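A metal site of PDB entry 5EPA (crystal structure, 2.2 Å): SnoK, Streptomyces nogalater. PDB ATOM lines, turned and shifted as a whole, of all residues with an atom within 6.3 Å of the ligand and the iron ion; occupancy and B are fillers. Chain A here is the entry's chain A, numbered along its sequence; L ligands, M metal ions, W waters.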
ATOM      1  N   TRP A  69     -29.392  20.574 -27.081  1.00  0.00           N
ATOM      2  CA  TRP A  69     -29.376  21.927 -27.574  1.00  0.00           C
ATOM      3  C   TRP A  69     -29.018  21.800 -29.034  1.00  0.00           C
ATOM      4  O   TRP A  69     -27.892  21.435 -29.383  1.00  0.00           O
ATOM      5  CB  TRP A  69     -28.354  22.746 -26.778  1.00  0.00           C
ATOM      6  CG  TRP A  69     -28.092  24.165 -27.174  1.00  0.00           C
ATOM      7  CD1 TRP A  69     -28.488  24.819 -28.301  1.00  0.00           C
ATOM      8  CD2 TRP A  69     -27.253  25.089 -26.440  1.00  0.00           C
ATOM      9  NE1 TRP A  69     -27.977  26.123 -28.310  1.00  0.00           N
ATOM     10  CE2 TRP A  69     -27.196  26.293 -27.186  1.00  0.00           C
ATOM     11  CE3 TRP A  69     -26.528  24.992 -25.249  1.00  0.00           C
ATOM     12  CZ2 TRP A  69     -26.469  27.413 -26.758  1.00  0.00           C
ATOM     13  CZ3 TRP A  69     -25.786  26.096 -24.819  1.00  0.00           C
ATOM     14  CH2 TRP A  69     -25.758  27.291 -25.576  1.00  0.00           C
ATOM     15  N   GLN A  77     -25.673  20.483 -30.955  1.00  0.00           N
ATOM     16  CA  GLN A  77     -24.610  21.411 -30.535  1.00  0.00           C
ATOM     17  C   GLN A  77     -24.062  21.050 -29.162  1.00  0.00           C
ATOM     18  O   GLN A  77     -22.858  20.998 -28.979  1.00  0.00           O
ATOM     19  CB  GLN A  77     -25.137  22.855 -30.518  1.00  0.00           C
ATOM     20  CG  GLN A  77     -25.585  23.308 -31.882  1.00  0.00           C
ATOM     21  CD  GLN A  77     -26.207  24.697 -31.892  1.00  0.00           C
ATOM     22  OE1 GLN A  77     -25.793  25.612 -31.191  1.00  0.00           O
ATOM     23  NE2 GLN A  77     -27.247  24.827 -32.695  1.00  0.00           N
ATOM     24  N   VAL A  78     -24.960  20.856 -28.186  1.00  0.00           N
ATOM     25  CA  VAL A  78     -24.575  20.553 -26.819  1.00  0.00           C
ATOM     26  C   VAL A  78     -25.599  19.633 -26.178  1.00  0.00           C
ATOM     27  O   VAL A  78     -26.805  19.758 -26.444  1.00  0.00           O
ATOM     28  CB  VAL A  78     -24.494  21.834 -25.984  1.00  0.00           C
ATOM     29  CG1 VAL A  78     -24.004  21.525 -24.600  1.00  0.00           C
ATOM     30  CG2 VAL A  78     -23.540  22.839 -26.593  1.00  0.00           C
ATOM     31  N   LEU A 120     -22.870  21.016 -19.442  1.00  0.00           N
ATOM     32  CA  LEU A 120     -22.677  21.337 -20.890  1.00  0.00           C
ATOM     33  C   LEU A 120     -21.652  20.414 -21.539  1.00  0.00           C
ATOM     34  O   LEU A 120     -20.438  20.596 -21.405  1.00  0.00           O
ATOM     35  CB  LEU A 120     -22.236  22.780 -21.061  1.00  0.00           C
ATOM     36  CG  LEU A 120     -23.202  23.853 -20.546  1.00  0.00           C
ATOM     37  CD1 LEU A 120     -22.405  25.133 -20.319  1.00  0.00           C
ATOM     38  CD2 LEU A 120     -24.387  24.072 -21.470  1.00  0.00           C
ATOM     39  N   VAL A 121     -22.169  19.400 -22.228  1.00  0.00           N
ATOM     40  CA  VAL A 121     -21.336  18.281 -22.726  1.00  0.00           C
ATOM     41  C   VAL A 121     -21.278  18.306 -24.227  1.00  0.00           C
ATOM     42  O   VAL A 121     -22.312  18.517 -24.882  1.00  0.00           O
ATOM     43  CB  VAL A 121     -21.908  16.914 -22.281  1.00  0.00           C
ATOM     44  CG1 VAL A 121     -21.316  15.772 -23.072  1.00  0.00           C
ATOM     45  CG2 VAL A 121     -21.618  16.683 -20.813  1.00  0.00           C
ATOM     46  N   LYS A 122     -20.088  18.111 -24.788  1.00  0.00           N
ATOM     47  CA  LYS A 122     -19.948  17.884 -26.238  1.00  0.00           C
ATOM     48  C   LYS A 122     -19.277  16.540 -26.499  1.00  0.00           C
ATOM     49  O   LYS A 122     -18.132  16.368 -26.128  1.00  0.00           O
ATOM     50  CB  LYS A 122     -19.148  19.003 -26.949  1.00  0.00           C
ATOM     51  CG  LYS A 122     -19.924  20.306 -27.197  1.00  0.00           C
ATOM     52  CD  LYS A 122     -19.075  21.267 -28.055  1.00  0.00           C
ATOM     53  CE  LYS A 122     -19.723  22.644 -28.258  1.00  0.00           C
ATOM     54  NZ  LYS A 122     -20.655  22.660 -29.408  1.00  0.00           N
ATOM     55  N   THR A 130     -21.362  25.334 -31.316  1.00  0.00           N
ATOM     56  CA  THR A 130     -22.420  26.057 -30.617  1.00  0.00           C
ATOM     57  C   THR A 130     -22.588  27.422 -31.307  1.00  0.00           C
ATOM     58  O   THR A 130     -21.680  28.247 -31.317  1.00  0.00           O
ATOM     59  CB  THR A 130     -22.100  26.278 -29.156  1.00  0.00           C
ATOM     60  OG1 THR A 130     -21.823  25.023 -28.521  1.00  0.00           O
ATOM     61  CG2 THR A 130     -23.274  26.925 -28.468  1.00  0.00           C
ATOM     62  N   HIS A 133     -24.046  33.658 -30.078  1.00  0.00           N
ATOM     63  CA  HIS A 133     -25.146  34.346 -29.398  1.00  0.00           C
ATOM     64  C   HIS A 133     -24.628  35.190 -28.269  1.00  0.00           C
ATOM     65  O   HIS A 133     -23.445  35.119 -27.940  1.00  0.00           O
ATOM     66  CB  HIS A 133     -26.155  33.316 -28.826  1.00  0.00           C
ATOM     67  CG  HIS A 133     -25.564  32.404 -27.771  1.00  0.00           C
ATOM     68  ND1 HIS A 133     -24.730  31.354 -28.078  1.00  0.00           N
ATOM     69  CD2 HIS A 133     -25.673  32.422 -26.414  1.00  0.00           C
ATOM     70  CE1 HIS A 133     -24.350  30.759 -26.947  1.00  0.00           C
ATOM     71  NE2 HIS A 133     -24.869  31.417 -25.911  1.00  0.00           N
ATOM     72  N   ASP A 134     -25.499  35.974 -27.660  1.00  0.00           N
ATOM     73  CA  ASP A 134     -25.238  36.484 -26.321  1.00  0.00           C
ATOM     74  C   ASP A 134     -26.276  35.859 -25.389  1.00  0.00           C
ATOM     75  O   ASP A 134     -27.247  35.272 -25.842  1.00  0.00           O
ATOM     76  CB  ASP A 134     -25.257  37.993 -26.227  1.00  0.00           C
ATOM     77  CG  ASP A 134     -26.639  38.634 -26.518  1.00  0.00           C
ATOM     78  OD1 ASP A 134     -27.682  38.102 -26.080  1.00  0.00           O
ATOM     79  OD2 ASP A 134     -26.647  39.705 -27.177  1.00  0.00           O
ATOM     80  N   ASP A 135     -26.010  35.887 -24.098  1.00  0.00           N
ATOM     81  CA  ASP A 135     -26.842  35.110 -23.152  1.00  0.00           C
ATOM     82  C   ASP A 135     -28.075  35.899 -22.775  1.00  0.00           C
ATOM     83  O   ASP A 135     -29.130  35.332 -22.557  1.00  0.00           O
ATOM     84  CB  ASP A 135     -26.034  34.734 -21.936  1.00  0.00           C
ATOM     85  CG  ASP A 135     -24.981  33.667 -22.219  1.00  0.00           C
ATOM     86  OD1 ASP A 135     -25.110  32.753 -23.117  1.00  0.00           O
ATOM     87  OD2 ASP A 135     -23.974  33.758 -21.488  1.00  0.00           O
ATOM     88  N   THR A 149     -21.668  34.860 -16.639  1.00  0.00           N
ATOM     89  CA  THR A 149     -21.634  33.407 -16.605  1.00  0.00           C
ATOM     90  C   THR A 149     -20.228  32.927 -16.309  1.00  0.00           C
ATOM     91  O   THR A 149     -19.262  33.484 -16.854  1.00  0.00           O
ATOM     92  CB  THR A 149     -22.041  32.806 -17.945  1.00  0.00           C
ATOM     93  OG1 THR A 149     -23.422  33.112 -18.255  1.00  0.00           O
ATOM     94  CG2 THR A 149     -21.850  31.294 -17.962  1.00  0.00           C
ATOM     95  N   ALA A 150     -20.119  31.957 -15.415  1.00  0.00           N
ATOM     96  CA  ALA A 150     -18.882  31.244 -15.166  1.00  0.00           C
ATOM     97  C   ALA A 150     -18.932  29.928 -15.931  1.00  0.00           C
ATOM     98  O   ALA A 150     -19.777  29.096 -15.673  1.00  0.00           O
ATOM     99  CB  ALA A 150     -18.735  30.952 -13.681  1.00  0.00           C
ATOM    100  N   TRP A 151     -18.025  29.746 -16.875  1.00  0.00           N
ATOM    101  CA  TRP A 151     -17.948  28.521 -17.679  1.00  0.00           C
ATOM    102  C   TRP A 151     -16.806  27.731 -17.141  1.00  0.00           C
ATOM    103  O   TRP A 151     -15.643  28.084 -17.336  1.00  0.00           O
ATOM    104  CB  TRP A 151     -17.739  28.893 -19.130  1.00  0.00           C
ATOM    105  CG  TRP A 151     -17.964  27.791 -20.145  1.00  0.00           C
ATOM    106  CD1 TRP A 151     -19.124  27.444 -20.740  1.00  0.00           C
ATOM    107  CD2 TRP A 151     -16.950  26.970 -20.727  1.00  0.00           C
ATOM    108  NE1 TRP A 151     -18.915  26.425 -21.641  1.00  0.00           N
ATOM    109  CE2 TRP A 151     -17.574  26.126 -21.642  1.00  0.00           C
ATOM    110  CE3 TRP A 151     -15.569  26.851 -20.521  1.00  0.00           C
ATOM    111  CZ2 TRP A 151     -16.874  25.208 -22.406  1.00  0.00           C
ATOM    112  CZ3 TRP A 151     -14.871  25.893 -21.254  1.00  0.00           C
ATOM    113  CH2 TRP A 151     -15.525  25.082 -22.173  1.00  0.00           C
ATOM    114  N   GLY A 162     -13.879  21.490 -28.537  1.00  0.00           N
ATOM    115  CA  GLY A 162     -15.076  22.303 -28.358  1.00  0.00           C
ATOM    116  C   GLY A 162     -14.920  23.514 -27.467  1.00  0.00           C
ATOM    117  O   GLY A 162     -15.771  23.807 -26.627  1.00  0.00           O
ATOM    118  N   MET A 164     -14.499  27.504 -26.192  1.00  0.00           N
ATOM    119  CA  MET A 164     -15.291  28.712 -26.393  1.00  0.00           C
ATOM    120  C   MET A 164     -14.493  29.759 -27.178  1.00  0.00           C
ATOM    121  O   MET A 164     -13.282  29.773 -27.089  1.00  0.00           O
ATOM    122  CB  MET A 164     -15.659  29.320 -25.043  1.00  0.00           C
ATOM    123  CG  MET A 164     -16.480  28.394 -24.149  1.00  0.00           C
ATOM    124  SD  MET A 164     -18.193  28.390 -24.655  1.00  0.00           S
ATOM    125  CE  MET A 164     -18.703  29.912 -23.897  1.00  0.00           C
ATOM    126  N   HIS A 216     -17.845  35.288 -18.637  1.00  0.00           N
ATOM    127  CA  HIS A 216     -18.261  36.245 -19.681  1.00  0.00           C
ATOM    128  C   HIS A 216     -19.566  36.957 -19.338  1.00  0.00           C
ATOM    129  O   HIS A 216     -20.529  36.359 -18.851  1.00  0.00           O
ATOM    130  CB  HIS A 216     -18.319  35.562 -21.110  1.00  0.00           C
ATOM    131  CG  HIS A 216     -19.404  34.539 -21.278  1.00  0.00           C
ATOM    132  ND1 HIS A 216     -19.210  33.216 -20.993  1.00  0.00           N
ATOM    133  CD2 HIS A 216     -20.705  34.659 -21.650  1.00  0.00           C
ATOM    134  CE1 HIS A 216     -20.340  32.551 -21.174  1.00  0.00           C
ATOM    135  NE2 HIS A 216     -21.240  33.397 -21.625  1.00  0.00           N
ATOM    136  N   HIS A 222     -20.536  35.279 -27.926  1.00  0.00           N
ATOM    137  CA  HIS A 222     -19.692  34.130 -27.856  1.00  0.00           C
ATOM    138  C   HIS A 222     -20.240  32.932 -28.617  1.00  0.00           C
ATOM    139  O   HIS A 222     -21.374  32.907 -29.077  1.00  0.00           O
ATOM    140  CB  HIS A 222     -19.467  33.761 -26.382  1.00  0.00           C
ATOM    141  CG  HIS A 222     -20.735  33.405 -25.646  1.00  0.00           C
ATOM    142  ND1 HIS A 222     -21.613  34.363 -25.193  1.00  0.00           N
ATOM    143  CD2 HIS A 222     -21.252  32.204 -25.253  1.00  0.00           C
ATOM    144  CE1 HIS A 222     -22.632  33.769 -24.572  1.00  0.00           C
ATOM    145  NE2 HIS A 222     -22.463  32.451 -24.615  1.00  0.00           N
ATOM    146  N   MET A 223     -19.411  31.900 -28.710  1.00  0.00           N
ATOM    147  CA  MET A 223     -19.746  30.724 -29.484  1.00  0.00           C
ATOM    148  C   MET A 223     -18.843  29.568 -29.013  1.00  0.00           C
ATOM    149  O   MET A 223     -17.996  29.779 -28.163  1.00  0.00           O
ATOM    150  CB  MET A 223     -19.577  31.035 -30.979  1.00  0.00           C
ATOM    151  CG  MET A 223     -18.118  31.131 -31.424  1.00  0.00           C
ATOM    152  SD  MET A 223     -17.903  32.258 -32.804  1.00  0.00           S
ATOM    153  CE  MET A 223     -17.924  33.829 -31.924  1.00  0.00           C
ATOM    154  N   ALA A 224     -19.000  28.375 -29.582  1.00  0.00           N
ATOM    155  CA  ALA A 224     -18.051  27.285 -29.335  1.00  0.00           C
ATOM    156  C   ALA A 224     -17.807  26.409 -30.533  1.00  0.00           C
ATOM    157  O   ALA A 224     -18.663  26.231 -31.348  1.00  0.00           O
ATOM    158  CB  ALA A 224     -18.522  26.430 -28.167  1.00  0.00           C
ATOM    159  N   GLU A 225     -16.624  25.815 -30.577  1.00  0.00           N
ATOM    160  CA  GLU A 225     -16.237  24.865 -31.623  1.00  0.00           C
ATOM    161  C   GLU A 225     -17.001  23.582 -31.515  1.00  0.00           C
ATOM    162  O   GLU A 225     -17.453  23.217 -30.449  1.00  0.00           O
ATOM    163  CB  GLU A 225     -14.775  24.429 -31.476  1.00  0.00           C
ATOM    164  CG  GLU A 225     -13.759  25.536 -31.523  1.00  0.00           C
ATOM    165  CD  GLU A 225     -13.887  26.337 -32.787  1.00  0.00           C
ATOM    166  OE1 GLU A 225     -13.630  25.758 -33.858  1.00  0.00           O
ATOM    167  OE2 GLU A 225     -14.278  27.536 -32.705  1.00  0.00           O
ATOM    168  N   ARG A 233     -16.029  16.498 -24.043  1.00  0.00           N
ATOM    169  CA  ARG A 233     -15.842  17.784 -23.342  1.00  0.00           C
ATOM    170  C   ARG A 233     -16.938  18.010 -22.337  1.00  0.00           C
ATOM    171  O   ARG A 233     -18.119  17.909 -22.683  1.00  0.00           O
ATOM    172  CB  ARG A 233     -15.920  18.969 -24.306  1.00  0.00           C
ATOM    173  CG  ARG A 233     -15.676  20.281 -23.619  1.00  0.00           C
ATOM    174  CD  ARG A 233     -16.329  21.429 -24.354  1.00  0.00           C
ATOM    175  NE  ARG A 233     -17.654  21.670 -23.849  1.00  0.00           N
ATOM    176  CZ  ARG A 233     -18.505  22.587 -24.284  1.00  0.00           C
ATOM    177  NH1 ARG A 233     -18.228  23.432 -25.302  1.00  0.00           N
ATOM    178  NH2 ARG A 233     -19.680  22.642 -23.703  1.00  0.00           N
ATOM    179  N   ALA A 235     -18.199  20.997 -19.618  1.00  0.00           N
ATOM    180  CA  ALA A 235     -18.146  22.180 -18.785  1.00  0.00           C
ATOM    181  C   ALA A 235     -19.412  22.291 -17.924  1.00  0.00           C
ATOM    182  O   ALA A 235     -20.410  21.605 -18.169  1.00  0.00           O
ATOM    183  CB  ALA A 235     -17.983  23.428 -19.645  1.00  0.00           C
ATOM    184  N   GLY A 237     -21.800  25.498 -16.741  1.00  0.00           N
ATOM    185  CA  GLY A 237     -22.045  26.919 -16.909  1.00  0.00           C
ATOM    186  C   GLY A 237     -22.914  27.393 -15.771  1.00  0.00           C
ATOM    187  O   GLY A 237     -23.984  26.878 -15.565  1.00  0.00           O
ATOM    188  N   VAL A 238     -22.459  28.398 -15.050  1.00  0.00           N
ATOM    189  CA  VAL A 238     -23.258  28.966 -13.962  1.00  0.00           C
ATOM    190  C   VAL A 238     -23.643  30.418 -14.289  1.00  0.00           C
ATOM    191  O   VAL A 238     -22.764  31.240 -14.490  1.00  0.00           O
ATOM    192  CB  VAL A 238     -22.479  28.960 -12.638  1.00  0.00           C
ATOM    193  CG1 VAL A 238     -23.362  29.464 -11.508  1.00  0.00           C
ATOM    194  CG2 VAL A 238     -22.007  27.590 -12.330  1.00  0.00           C
HETATM  195  C1  LIG L   1     -22.599  29.705 -22.246  1.00  0.00           C
HETATM  196  O1  LIG L   1     -22.006  29.252 -21.227  1.00  0.00           O
HETATM  197  O2  LIG L   1     -23.291  30.758 -22.298  1.00  0.00           O
HETATM  198  C2  LIG L   1     -22.554  28.958 -23.492  1.00  0.00           C
HETATM  199  O3  LIG L   1     -23.151  29.487 -24.412  1.00  0.00           O
HETATM  200  C3  LIG L   1     -21.801  27.647 -23.603  1.00  0.00           C
HETATM  201  C4  LIG L   1     -21.993  26.859 -24.900  1.00  0.00           C
HETATM  202  C5  LIG L   1     -21.112  25.592 -24.875  1.00  0.00           C
HETATM  203  O4  LIG L   1     -20.713  25.069 -23.788  1.00  0.00           O
HETATM  204  O5  LIG L   1     -20.789  25.060 -25.945  1.00  0.00           O
HETATM  205 FE    FE M   1     -24.133  31.297 -23.927  1.00  0.00          FE
HETATM  206  O   HOH W   1     -24.038  28.796 -19.091  1.00  0.00           O
HETATM  207  O   HOH W   2     -24.871  31.380 -20.047  1.00  0.00           O
HETATM  208  O   HOH W   3     -25.148  28.053 -21.384  1.00  0.00           O
HETATM  209  O   HOH W   4     -25.844  30.131 -23.314  1.00  0.00           O
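The side-chain hydroxyl (OG1) of Thr 130 lies within hydrogen-bond range of an oxygen (O5) of the ligand (2.8 Å).
NE1 of Trp 151 is in hydrogen-bond range of O4 of the ligand.
NE2 of His 216 lies close to O2 of the ligand, 3.4 Å away.
NH2 of Arg 233 lies within salt-bridge range of O4 of the ligand (2.6 Å).
NE2 of His 216 lies close to NE2 of His 222, at 3.4 Å.
The backbone NH (N) of Leu 120 lies within hydrogen-bond range of the backbone carbonyl oxygen (O) of Ala 235 (2.8 Å).
OG1 of Thr 130 is in hydrogen-bond range of NZ of Lys 122.
The backbone carbonyl oxygen (O) of Gly 162 sits at hydrogen-bond distance from the guanidinium group (NH1) of Arg 233.
N of Thr 149 is in hydrogen-bond range of O of His 216, at 2.9 Å.
N of Trp 69 lies within hydrogen-bond range of O of Val 78, at 2.8 Å.
NE2 of His 216 lies within hydrogen-bond range of OD2 of Asp 135, 2.8 Å away.
SD of Met 164 is in hydrogen-bond range of NE1 of Trp 151 (3.7 Å).
Merely in contact with the ligand: Trp 69 (3.6 Å), Val 78 (3.6 Å), Leu 120 (3.9 Å), Lys 122 (3.5 Å), Thr 149 (3.9 Å), Met 164 (3.8 Å) and Ala 224 (3.5 Å).
Of the 24 residues printed, 14 come within 4 Å of the ligand.
Along chain A the residues within 4 Å of the ligand span positions 69 to 233.
The nearest printed residue that does not touch the ligand is Gly 237 (4.9 Å).
Three residues have an atom within 4 Å of the iron ion: His 133, Asp 135 and His 222.
The iron ion is bound by O2 of the ligand, OD1 of Asp 135, O3 of the ligand, NE2 of His 133, NE2 of His 222 and water W4.
Water W2 bridges the side-chain hydroxyl (OG1) of Thr 149 (2.9 Å) and the side-chain carboxylate (OD2) of Asp 135 (2.9 Å).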
